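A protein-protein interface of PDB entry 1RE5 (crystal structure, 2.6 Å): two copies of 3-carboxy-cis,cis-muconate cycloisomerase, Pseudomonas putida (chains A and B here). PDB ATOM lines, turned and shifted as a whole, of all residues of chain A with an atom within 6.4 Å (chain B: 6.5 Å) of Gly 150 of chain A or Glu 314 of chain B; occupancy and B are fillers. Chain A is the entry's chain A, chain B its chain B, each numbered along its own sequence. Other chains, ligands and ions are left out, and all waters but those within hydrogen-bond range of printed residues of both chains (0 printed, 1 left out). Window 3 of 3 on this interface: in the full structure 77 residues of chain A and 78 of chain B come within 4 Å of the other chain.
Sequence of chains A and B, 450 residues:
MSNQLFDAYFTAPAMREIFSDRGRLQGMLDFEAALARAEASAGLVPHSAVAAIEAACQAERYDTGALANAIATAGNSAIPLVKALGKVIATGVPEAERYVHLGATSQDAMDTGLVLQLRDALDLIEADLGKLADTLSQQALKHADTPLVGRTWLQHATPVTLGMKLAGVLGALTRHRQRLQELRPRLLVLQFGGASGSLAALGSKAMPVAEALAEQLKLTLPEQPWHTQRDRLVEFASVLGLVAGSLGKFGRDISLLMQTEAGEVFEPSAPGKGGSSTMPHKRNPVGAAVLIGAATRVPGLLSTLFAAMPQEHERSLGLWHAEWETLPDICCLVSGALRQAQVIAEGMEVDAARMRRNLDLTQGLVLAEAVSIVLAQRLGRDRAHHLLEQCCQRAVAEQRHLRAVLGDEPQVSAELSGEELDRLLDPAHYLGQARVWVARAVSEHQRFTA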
ATOM      1  N   LEU A 148     -15.900 -22.372 -14.202  1.00  0.00           N
ATOM      2  CA  LEU A 148     -17.297 -22.715 -14.454  1.00  0.00           C
ATOM      3  C   LEU A 148     -17.904 -22.898 -13.057  1.00  0.00           C
ATOM      4  O   LEU A 148     -17.177 -23.167 -12.099  1.00  0.00           O
ATOM      5  CB  LEU A 148     -17.453 -23.989 -15.338  1.00  0.00           C
ATOM      6  CG  LEU A 148     -17.089 -25.463 -15.046  1.00  0.00           C
ATOM      7  CD1 LEU A 148     -17.453 -26.378 -16.204  1.00  0.00           C
ATOM      8  CD2 LEU A 148     -15.622 -25.562 -14.826  1.00  0.00           C
ATOM      9  N   VAL A 149     -19.216 -22.696 -12.930  1.00  0.00           N
ATOM     10  CA  VAL A 149     -19.892 -22.829 -11.639  1.00  0.00           C
ATOM     11  C   VAL A 149     -19.908 -24.285 -11.183  1.00  0.00           C
ATOM     12  O   VAL A 149     -19.978 -25.196 -12.007  1.00  0.00           O
ATOM     13  CB  VAL A 149     -21.372 -22.325 -11.709  1.00  0.00           C
ATOM     14  CG1 VAL A 149     -22.185 -23.202 -12.640  1.00  0.00           C
ATOM     15  CG2 VAL A 149     -22.006 -22.337 -10.324  1.00  0.00           C
ATOM     16  N   GLY A 150     -19.834 -24.510  -9.876  1.00  0.00           N
ATOM     17  CA  GLY A 150     -19.880 -25.872  -9.390  1.00  0.00           C
ATOM     18  C   GLY A 150     -21.336 -26.300  -9.293  1.00  0.00           C
ATOM     19  O   GLY A 150     -22.199 -25.491  -8.957  1.00  0.00           O
ATOM     20  N   ARG A 151     -21.628 -27.561  -9.585  1.00  0.00           N
ATOM     21  CA  ARG A 151     -22.998 -28.029  -9.506  1.00  0.00           C
ATOM     22  C   ARG A 151     -23.145 -29.199  -8.533  1.00  0.00           C
ATOM     23  O   ARG A 151     -22.592 -30.286  -8.719  1.00  0.00           O
ATOM     24  CB  ARG A 151     -23.495 -28.403 -10.897  1.00  0.00           C
ATOM     25  CG  ARG A 151     -23.341 -27.262 -11.876  1.00  0.00           C
ATOM     26  CD  ARG A 151     -23.813 -27.602 -13.288  1.00  0.00           C
ATOM     27  NE  ARG A 151     -23.032 -26.858 -14.281  1.00  0.00           N
ATOM     28  CZ  ARG A 151     -23.425 -25.730 -14.863  1.00  0.00           C
ATOM     29  NH1 ARG A 151     -24.606 -25.198 -14.568  1.00  0.00           N
ATOM     30  NH2 ARG A 151     -22.622 -25.126 -15.727  1.00  0.00           N
ATOM     31  N   THR A 152     -23.919 -28.941  -7.490  1.00  0.00           N
ATOM     32  CA  THR A 152     -24.183 -29.877  -6.417  1.00  0.00           C
ATOM     33  C   THR A 152     -25.675 -30.210  -6.409  1.00  0.00           C
ATOM     34  O   THR A 152     -26.492 -29.308  -6.276  1.00  0.00           O
ATOM     35  CB  THR A 152     -23.773 -29.202  -5.113  1.00  0.00           C
ATOM     36  OG1 THR A 152     -22.357 -29.327  -4.965  1.00  0.00           O
ATOM     37  CG2 THR A 152     -24.498 -29.788  -3.920  1.00  0.00           C
ATOM     38  N   TRP A 153     -26.041 -31.487  -6.538  1.00  0.00           N
ATOM     39  CA  TRP A 153     -27.462 -31.868  -6.574  1.00  0.00           C
ATOM     40  C   TRP A 153     -28.154 -31.061  -7.672  1.00  0.00           C
ATOM     41  O   TRP A 153     -29.342 -30.737  -7.556  1.00  0.00           O
ATOM     42  CB  TRP A 153     -28.159 -31.552  -5.245  1.00  0.00           C
ATOM     43  CG  TRP A 153     -27.728 -32.383  -4.067  1.00  0.00           C
ATOM     44  CD1 TRP A 153     -26.455 -32.548  -3.597  1.00  0.00           C
ATOM     45  CD2 TRP A 153     -28.583 -33.086  -3.155  1.00  0.00           C
ATOM     46  NE1 TRP A 153     -26.464 -33.303  -2.445  1.00  0.00           N
ATOM     47  CE2 TRP A 153     -27.757 -33.646  -2.152  1.00  0.00           C
ATOM     48  CE3 TRP A 153     -29.967 -33.295  -3.087  1.00  0.00           C
ATOM     49  CZ2 TRP A 153     -28.270 -34.395  -1.089  1.00  0.00           C
ATOM     50  CZ3 TRP A 153     -30.479 -34.047  -2.022  1.00  0.00           C
ATOM     51  CH2 TRP A 153     -29.627 -34.586  -1.039  1.00  0.00           C
ATOM     52  N   GLN A 155     -27.626 -28.038  -8.363  1.00  0.00           N
ATOM     53  CA  GLN A 155     -27.764 -26.651  -7.908  1.00  0.00           C
ATOM     54  C   GLN A 155     -26.392 -25.981  -7.948  1.00  0.00           C
ATOM     55  O   GLN A 155     -25.361 -26.631  -7.734  1.00  0.00           O
ATOM     56  CB  GLN A 155     -28.270 -26.604  -6.477  1.00  0.00           C
ATOM     57  CG  GLN A 155     -29.550 -27.342  -6.274  1.00  0.00           C
ATOM     58  CD  GLN A 155     -30.716 -26.605  -6.863  1.00  0.00           C
ATOM     59  OE1 GLN A 155     -31.096 -25.530  -6.380  1.00  0.00           O
ATOM     60  NE2 GLN A 155     -31.297 -27.167  -7.919  1.00  0.00           N
ATOM     61  N   HIS A 156     -26.384 -24.679  -8.216  1.00  0.00           N
ATOM     62  CA  HIS A 156     -25.142 -23.919  -8.287  1.00  0.00           C
ATOM     63  C   HIS A 156     -24.424 -23.904  -6.940  1.00  0.00           C
ATOM     64  O   HIS A 156     -25.054 -23.750  -5.897  1.00  0.00           O
ATOM     65  CB  HIS A 156     -25.452 -22.501  -8.766  1.00  0.00           C
ATOM     66  CG  HIS A 156     -25.592 -22.395 -10.254  1.00  0.00           C
ATOM     67  ND1 HIS A 156     -25.964 -23.464 -11.043  1.00  0.00           N
ATOM     68  CD2 HIS A 156     -25.367 -21.364 -11.102  1.00  0.00           C
ATOM     69  CE1 HIS A 156     -25.953 -23.097 -12.312  1.00  0.00           C
ATOM     70  NE2 HIS A 156     -25.594 -21.829 -12.376  1.00  0.00           N
ATOM     71  N   ALA A 157     -23.108 -24.089  -6.975  1.00  0.00           N
ATOM     72  CA  ALA A 157     -22.270 -24.099  -5.777  1.00  0.00           C
ATOM     73  C   ALA A 157     -20.988 -23.355  -6.103  1.00  0.00           C
ATOM     74  O   ALA A 157     -20.804 -22.922  -7.241  1.00  0.00           O
ATOM     75  CB  ALA A 157     -21.942 -25.523  -5.373  1.00  0.00           C
ATOM     76  N   THR A 158     -20.099 -23.218  -5.123  1.00  0.00           N
ATOM     77  CA  THR A 158     -18.849 -22.507  -5.351  1.00  0.00           C
ATOM     78  C   THR A 158     -18.144 -22.924  -6.644  1.00  0.00           C
ATOM     79  O   THR A 158     -18.274 -24.054  -7.109  1.00  0.00           O
ATOM     80  CB  THR A 158     -17.884 -22.677  -4.172  1.00  0.00           C
ATOM     81  OG1 THR A 158     -17.743 -24.067  -3.862  1.00  0.00           O
ATOM     82  CG2 THR A 158     -18.404 -21.935  -2.956  1.00  0.00           C
ATOM     83  N   PRO A 159     -17.388 -22.002  -7.243  1.00  0.00           N
ATOM     84  CA  PRO A 159     -16.656 -22.237  -8.486  1.00  0.00           C
ATOM     85  C   PRO A 159     -15.833 -23.505  -8.529  1.00  0.00           C
ATOM     86  O   PRO A 159     -15.461 -24.077  -7.499  1.00  0.00           O
ATOM     87  CB  PRO A 159     -15.789 -20.992  -8.618  1.00  0.00           C
ATOM     88  CG  PRO A 159     -16.642 -19.935  -8.014  1.00  0.00           C
ATOM     89  CD  PRO A 159     -17.161 -20.627  -6.763  1.00  0.00           C
ATOM     90  N   VAL A 160     -15.540 -23.906  -9.758  1.00  0.00           N
ATOM     91  CA  VAL A 160     -14.770 -25.091 -10.075  1.00  0.00           C
ATOM     92  C   VAL A 160     -14.143 -24.742 -11.425  1.00  0.00           C
ATOM     93  O   VAL A 160     -14.494 -23.719 -12.013  1.00  0.00           O
ATOM     94  CB  VAL A 160     -15.725 -26.304 -10.185  1.00  0.00           C
ATOM     95  CG1 VAL A 160     -15.344 -27.196 -11.353  1.00  0.00           C
ATOM     96  CG2 VAL A 160     -15.701 -27.081  -8.894  1.00  0.00           C
ATOM     97  N   LYS A 165     -12.639 -30.809 -13.484  1.00  0.00           N
ATOM     98  CA  LYS A 165     -13.578 -31.853 -13.863  1.00  0.00           C
ATOM     99  C   LYS A 165     -12.899 -32.900 -14.734  1.00  0.00           C
ATOM    100  O   LYS A 165     -12.914 -34.081 -14.398  1.00  0.00           O
ATOM    101  CB  LYS A 165     -14.772 -31.257 -14.609  1.00  0.00           C
ATOM    102  CG  LYS A 165     -15.590 -30.246 -13.787  1.00  0.00           C
ATOM    103  CD  LYS A 165     -16.789 -29.718 -14.566  1.00  0.00           C
ATOM    104  CE  LYS A 165     -17.912 -30.733 -14.608  1.00  0.00           C
ATOM    105  NZ  LYS A 165     -18.631 -30.793 -13.308  1.00  0.00           N
ATOM    106  N   LYS A 249     -19.982 -41.553 -16.377  1.00  0.00           N
ATOM    107  CA  LYS A 249     -20.041 -40.301 -15.632  1.00  0.00           C
ATOM    108  C   LYS A 249     -19.669 -39.165 -16.577  1.00  0.00           C
ATOM    109  O   LYS A 249     -20.314 -38.113 -16.594  1.00  0.00           O
ATOM    110  CB  LYS A 249     -19.063 -40.347 -14.450  1.00  0.00           C
ATOM    111  CG  LYS A 249     -19.194 -39.189 -13.448  1.00  0.00           C
ATOM    112  CD  LYS A 249     -18.138 -38.127 -13.656  1.00  0.00           C
ATOM    113  CE  LYS A 249     -18.043 -37.172 -12.457  1.00  0.00           C
ATOM    114  NZ  LYS A 249     -19.214 -36.260 -12.272  1.00  0.00           N
ATOM    115  N   ASP A 253     -22.009 -35.934 -17.779  1.00  0.00           N
ATOM    116  CA  ASP A 253     -21.564 -34.564 -17.599  1.00  0.00           C
ATOM    117  C   ASP A 253     -21.605 -33.781 -18.899  1.00  0.00           C
ATOM    118  O   ASP A 253     -22.031 -32.626 -18.907  1.00  0.00           O
ATOM    119  CB  ASP A 253     -20.159 -34.551 -16.984  1.00  0.00           C
ATOM    120  CG  ASP A 253     -20.176 -34.898 -15.490  1.00  0.00           C
ATOM    121  OD1 ASP A 253     -21.282 -34.999 -14.907  1.00  0.00           O
ATOM    122  OD2 ASP A 253     -19.091 -35.060 -14.890  1.00  0.00           O
ATOM    123  N   LEU A 359     -22.244 -18.301 -14.436  1.00  0.00           N
ATOM    124  CA  LEU A 359     -21.699 -18.158 -13.091  1.00  0.00           C
ATOM    125  C   LEU A 359     -22.451 -17.164 -12.214  1.00  0.00           C
ATOM    126  O   LEU A 359     -22.685 -17.450 -11.036  1.00  0.00           O
ATOM    127  CB  LEU A 359     -20.211 -17.805 -13.148  1.00  0.00           C
ATOM    128  CG  LEU A 359     -19.286 -18.974 -12.800  1.00  0.00           C
ATOM    129  CD1 LEU A 359     -17.884 -18.723 -13.331  1.00  0.00           C
ATOM    130  CD2 LEU A 359     -19.266 -19.170 -11.295  1.00  0.00           C
ATOM    131  N   VAL A 366     -23.459 -17.234  -4.926  1.00  0.00           N
ATOM    132  CA  VAL A 366     -22.650 -18.440  -4.900  1.00  0.00           C
ATOM    133  C   VAL A 366     -21.235 -18.102  -4.424  1.00  0.00           C
ATOM    134  O   VAL A 366     -20.428 -18.991  -4.143  1.00  0.00           O
ATOM    135  CB  VAL A 366     -22.593 -19.091  -6.319  1.00  0.00           C
ATOM    136  CG1 VAL A 366     -21.397 -18.564  -7.114  1.00  0.00           C
ATOM    137  CG2 VAL A 366     -22.551 -20.600  -6.202  1.00  0.00           C
ATOM    138  N   GLN B 107     -20.579 -34.624   2.496  1.00  0.00           N
ATOM    139  CA  GLN B 107     -19.997 -35.819   1.887  1.00  0.00           C
ATOM    140  C   GLN B 107     -18.580 -36.125   2.370  1.00  0.00           C
ATOM    141  O   GLN B 107     -18.172 -37.289   2.390  1.00  0.00           O
ATOM    142  CB  GLN B 107     -20.016 -35.726   0.350  1.00  0.00           C
ATOM    143  CG  GLN B 107     -19.707 -37.072  -0.317  1.00  0.00           C
ATOM    144  CD  GLN B 107     -19.824 -37.059  -1.834  1.00  0.00           C
ATOM    145  OE1 GLN B 107     -19.678 -38.094  -2.485  1.00  0.00           O
ATOM    146  NE2 GLN B 107     -20.091 -35.896  -2.400  1.00  0.00           N
ATOM    147  N   ALA B 195     -17.514 -28.085  -0.147  1.00  0.00           N
ATOM    148  CA  ALA B 195     -18.677 -27.786  -0.986  1.00  0.00           C
ATOM    149  C   ALA B 195     -18.655 -28.263  -2.444  1.00  0.00           C
ATOM    150  O   ALA B 195     -19.608 -28.896  -2.895  1.00  0.00           O
ATOM    151  CB  ALA B 195     -18.947 -26.306  -0.951  1.00  0.00           C
ATOM    152  N   SER B 196     -17.603 -27.946  -3.193  1.00  0.00           N
ATOM    153  CA  SER B 196     -17.528 -28.395  -4.584  1.00  0.00           C
ATOM    154  C   SER B 196     -16.201 -29.092  -4.922  1.00  0.00           C
ATOM    155  O   SER B 196     -15.859 -29.253  -6.100  1.00  0.00           O
ATOM    156  CB  SER B 196     -17.747 -27.217  -5.544  1.00  0.00           C
ATOM    157  OG  SER B 196     -16.632 -26.333  -5.557  1.00  0.00           O
ATOM    158  N   GLY B 197     -15.462 -29.499  -3.890  1.00  0.00           N
ATOM    159  CA  GLY B 197     -14.193 -30.174  -4.092  1.00  0.00           C
ATOM    160  C   GLY B 197     -13.015 -29.256  -4.366  1.00  0.00           C
ATOM    161  O   GLY B 197     -11.929 -29.725  -4.721  1.00  0.00           O
ATOM    162  N   HIS B 227     -15.756 -37.006  -4.817  1.00  0.00           N
ATOM    163  CA  HIS B 227     -17.183 -36.978  -4.504  1.00  0.00           C
ATOM    164  C   HIS B 227     -18.035 -37.700  -5.540  1.00  0.00           C
ATOM    165  O   HIS B 227     -19.049 -38.285  -5.188  1.00  0.00           O
ATOM    166  CB  HIS B 227     -17.692 -35.537  -4.380  1.00  0.00           C
ATOM    167  CG  HIS B 227     -17.064 -34.756  -3.262  1.00  0.00           C
ATOM    168  ND1 HIS B 227     -16.868 -35.283  -2.000  1.00  0.00           N
ATOM    169  CD2 HIS B 227     -16.639 -33.473  -3.201  1.00  0.00           C
ATOM    170  CE1 HIS B 227     -16.347 -34.359  -1.214  1.00  0.00           C
ATOM    171  NE2 HIS B 227     -16.199 -33.252  -1.917  1.00  0.00           N
ATOM    172  N   THR B 228     -17.639 -37.652  -6.815  1.00  0.00           N
ATOM    173  CA  THR B 228     -18.411 -38.315  -7.867  1.00  0.00           C
ATOM    174  C   THR B 228     -17.640 -39.337  -8.708  1.00  0.00           C
ATOM    175  O   THR B 228     -18.091 -39.741  -9.780  1.00  0.00           O
ATOM    176  CB  THR B 228     -19.067 -37.295  -8.821  1.00  0.00           C
ATOM    177  OG1 THR B 228     -18.062 -36.441  -9.383  1.00  0.00           O
ATOM    178  CG2 THR B 228     -20.100 -36.463  -8.064  1.00  0.00           C
ATOM    179  N   GLN B 311     -22.366 -40.551 -11.648  1.00  0.00           N
ATOM    180  CA  GLN B 311     -22.870 -39.475 -10.809  1.00  0.00           C
ATOM    181  C   GLN B 311     -22.513 -38.112 -11.401  1.00  0.00           C
ATOM    182  O   GLN B 311     -21.349 -37.828 -11.688  1.00  0.00           O
ATOM    183  CB  GLN B 311     -22.317 -39.624  -9.394  1.00  0.00           C
ATOM    184  CG  GLN B 311     -22.304 -41.067  -8.907  1.00  0.00           C
ATOM    185  CD  GLN B 311     -22.246 -41.180  -7.399  1.00  0.00           C
ATOM    186  OE1 GLN B 311     -21.769 -40.268  -6.725  1.00  0.00           O
ATOM    187  NE2 GLN B 311     -22.728 -42.307  -6.857  1.00  0.00           N
ATOM    188  N   GLU B 312     -23.532 -37.272 -11.567  1.00  0.00           N
ATOM    189  CA  GLU B 312     -23.380 -35.955 -12.172  1.00  0.00           C
ATOM    190  C   GLU B 312     -22.625 -34.880 -11.414  1.00  0.00           C
ATOM    191  O   GLU B 312     -22.826 -34.660 -10.214  1.00  0.00           O
ATOM    192  CB  GLU B 312     -24.753 -35.411 -12.551  1.00  0.00           C
ATOM    193  CG  GLU B 312     -25.897 -36.345 -12.181  1.00  0.00           C
ATOM    194  CD  GLU B 312     -26.463 -36.064 -10.810  1.00  0.00           C
ATOM    195  OE1 GLU B 312     -27.369 -36.817 -10.377  1.00  0.00           O
ATOM    196  OE2 GLU B 312     -26.013 -35.085 -10.173  1.00  0.00           O
ATOM    197  N   HIS B 313     -21.752 -34.208 -12.159  1.00  0.00           N
ATOM    198  CA  HIS B 313     -20.950 -33.098 -11.666  1.00  0.00           C
ATOM    199  C   HIS B 313     -20.234 -33.265 -10.323  1.00  0.00           C
ATOM    200  O   HIS B 313     -19.518 -34.231 -10.106  1.00  0.00           O
ATOM    201  CB  HIS B 313     -21.809 -31.816 -11.633  1.00  0.00           C
ATOM    202  CG  HIS B 313     -22.348 -31.414 -12.971  1.00  0.00           C
ATOM    203  ND1 HIS B 313     -21.544 -31.261 -14.082  1.00  0.00           N
ATOM    204  CD2 HIS B 313     -23.609 -31.128 -13.376  1.00  0.00           C
ATOM    205  CE1 HIS B 313     -22.288 -30.899 -15.114  1.00  0.00           C
ATOM    206  NE2 HIS B 313     -23.545 -30.812 -14.712  1.00  0.00           N
ATOM    207  N   GLU B 314     -20.440 -32.297  -9.432  1.00  0.00           N
ATOM    208  CA  GLU B 314     -19.794 -32.258  -8.130  1.00  0.00           C
ATOM    209  C   GLU B 314     -20.451 -33.054  -6.998  1.00  0.00           C
ATOM    210  O   GLU B 314     -19.835 -33.297  -5.954  1.00  0.00           O
ATOM    211  CB  GLU B 314     -19.617 -30.795  -7.721  1.00  0.00           C
ATOM    212  CG  GLU B 314     -18.580 -30.038  -8.567  1.00  0.00           C
ATOM    213  CD  GLU B 314     -18.922 -29.988 -10.063  1.00  0.00           C
ATOM    214  OE1 GLU B 314     -20.006 -29.468 -10.424  1.00  0.00           O
ATOM    215  OE2 GLU B 314     -18.091 -30.457 -10.879  1.00  0.00           O
ATOM    216  N   ARG B 315     -21.699 -33.445  -7.194  1.00  0.00           N
ATOM    217  CA  ARG B 315     -22.402 -34.243  -6.202  1.00  0.00           C
ATOM    218  C   ARG B 315     -23.699 -34.656  -6.849  1.00  0.00           C
ATOM    219  O   ARG B 315     -24.449 -33.816  -7.336  1.00  0.00           O
ATOM    220  CB  ARG B 315     -22.681 -33.451  -4.928  1.00  0.00           C
ATOM    221  CG  ARG B 315     -22.890 -34.340  -3.705  1.00  0.00           C
ATOM    222  CD  ARG B 315     -23.040 -33.522  -2.447  1.00  0.00           C
ATOM    223  NE  ARG B 315     -22.134 -32.364  -2.443  1.00  0.00           N
ATOM    224  CZ  ARG B 315     -20.806 -32.434  -2.371  1.00  0.00           C
ATOM    225  NH1 ARG B 315     -20.204 -33.603  -2.282  1.00  0.00           N
ATOM    226  NH2 ARG B 315     -20.072 -31.337  -2.429  1.00  0.00           N
ATOM    227  N   SER B 316     -23.953 -35.956  -6.855  1.00  0.00           N
ATOM    228  CA  SER B 316     -25.145 -36.510  -7.481  1.00  0.00           C
ATOM    229  C   SER B 316     -26.238 -36.888  -6.491  1.00  0.00           C
ATOM    230  O   SER B 316     -25.938 -37.446  -5.441  1.00  0.00           O
ATOM    231  CB  SER B 316     -24.730 -37.742  -8.286  1.00  0.00           C
ATOM    232  OG  SER B 316     -25.816 -38.618  -8.474  1.00  0.00           O
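The side-chain hydroxyl (OG1) of Thr 158 of chain A is in hydrogen-bond range of the side-chain hydroxyl (OG) of Ser 196 of chain B, 3.0 Å away. The side-chain amino group (NZ) of Lys 165 of chain A is in salt-bridge range of the side-chain carboxylate (OE2) of Glu 314 of chain B, at 2.5 Å. The side-chain amino group (NZ) of Lys 249 of chain A sits at hydrogen-bond distance from the side-chain hydroxyl (OG1) of Thr 228 of chain B. OE1 of Glu 314 of chain B sits at hydrogen-bond distance from N of Arg 151 of chain A (2.6 Å). ND1 of His 313 of chain B is in hydrogen-bond range of NZ of Lys 165 of chain A. OG1 of Thr 152 of chain A sits at hydrogen-bond distance from O of Ala 195 of chain B, at 3.5 Å. The backbone NH (N) of His 313 of chain B is in hydrogen-bond range of the side-chain carboxylate (OD1) of Asp 253 of chain A (2.9 Å). The backbone carbonyl oxygen of Arg 315 of chain B sits at hydrogen-bond distance from the backbone NH of Trp 153 of chain A, at 2.9 Å. O of Pro 159 of chain A sits at hydrogen-bond distance from OG of Ser 196 of chain B. The side-chain amino group (NZ) of Lys 249 of chain A is in hydrogen-bond range of the backbone carbonyl oxygen (O) of His 313 of chain B. The side-chain amino group (NZ) of Lys 249 of chain A sits at hydrogen-bond distance from the backbone carbonyl oxygen (O) of Gln 311 of chain B (2.7 Å).
No position is printed for both chains.
Of the 12 printed residues of chain B, 8 touch a printed residue of chain A. Printed residues of chain B that touch a printed residue of chain A: Ala 195, Ser 196, Thr 228, Gln 311, Glu 312, His 313, Glu 314 and Arg 315. Hydrophobic or aromatic side chains of chain B within 4 Å of the printed part of chain A: Ala 195 and His 313. Hydrophobic or aromatic side chains of chain A that line the printed part of chain B: Trp 153 and Val 160. Along chain A the printed residues that touch a printed residue of chain B span positions 150 to 253. Among the printed residues, Asp or Glu carboxylates within 4 Å of a Lys or Arg side-chain nitrogen of the other chain: Lys 165 of chain A with Glu 314 of chain B (2.5 Å).
Gly 150 of chain A touches Glu 314 of chain B. Arg 151 of chain A touches His 313 of chain B (O to CB, 3.4 Å). O of Arg 151 of chain A touches N of Arg 315 of chain B, at 3.6 Å. Arg 315 of chain B touches Thr 152 of chain A. Thr 158 of chain A touches Ala 195 of chain B. O of Ser 196 of chain B touches CG2 of Val 160 of chain A, 3.5 Å away. Lys 249 of chain A touches Glu 312 of chain B (NZ to C, 3.8 Å). Asp 253 of chain A touches Glu 312 of chain B (OD1 to CA, 3.6 Å).
The backbone NH (N) of Ala 157 of chain A sits at hydrogen-bond distance from the backbone carbonyl oxygen (O) of Gly 150 of chain A, at 2.6 Å. OG1 of Thr 228 of chain B is in hydrogen-bond range of O of His 313 of chain B (2.7 Å). The backbone NH (N) of Gly 150 of chain A is in hydrogen-bond range of the backbone carbonyl oxygen (O) of Thr 158 of chain A (3.2 Å). O of Ala 195 of chain B sits at hydrogen-bond distance from NH2 of Arg 315 of chain B. OE1 of Glu 312 of chain B lies within hydrogen-bond range of OG of Ser 316 of chain B (3.0 Å). The backbone NH (N) of Leu 148 of chain A lies within hydrogen-bond range of the backbone carbonyl oxygen (O) of Val 160 of chain A, at 2.9 Å.
Of the printed residues of chain B, Thr 152 of chain A touches Ala 195 and Arg 315. Gln 107 of chain B touches none of the printed residues of chain A. Of the printed residues of chain A, Ala 195 of chain B touches Thr 152 and Thr 158. Gly 197 of chain B touches none of the printed residues of chain A. Of the printed residues of chain A, Arg 315 of chain B touches Arg 151 (3.6 Å), Thr 152 (3.8 Å) and Trp 153 (2.9 Å). The nearest residue of chain B that does not touch Gly 150 of chain A is Ser 196 of chain B (4.6 Å). The nearest printed residue of chain A that does not touch Glu 314 of chain B is Val 160 of chain A (4.1 Å).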
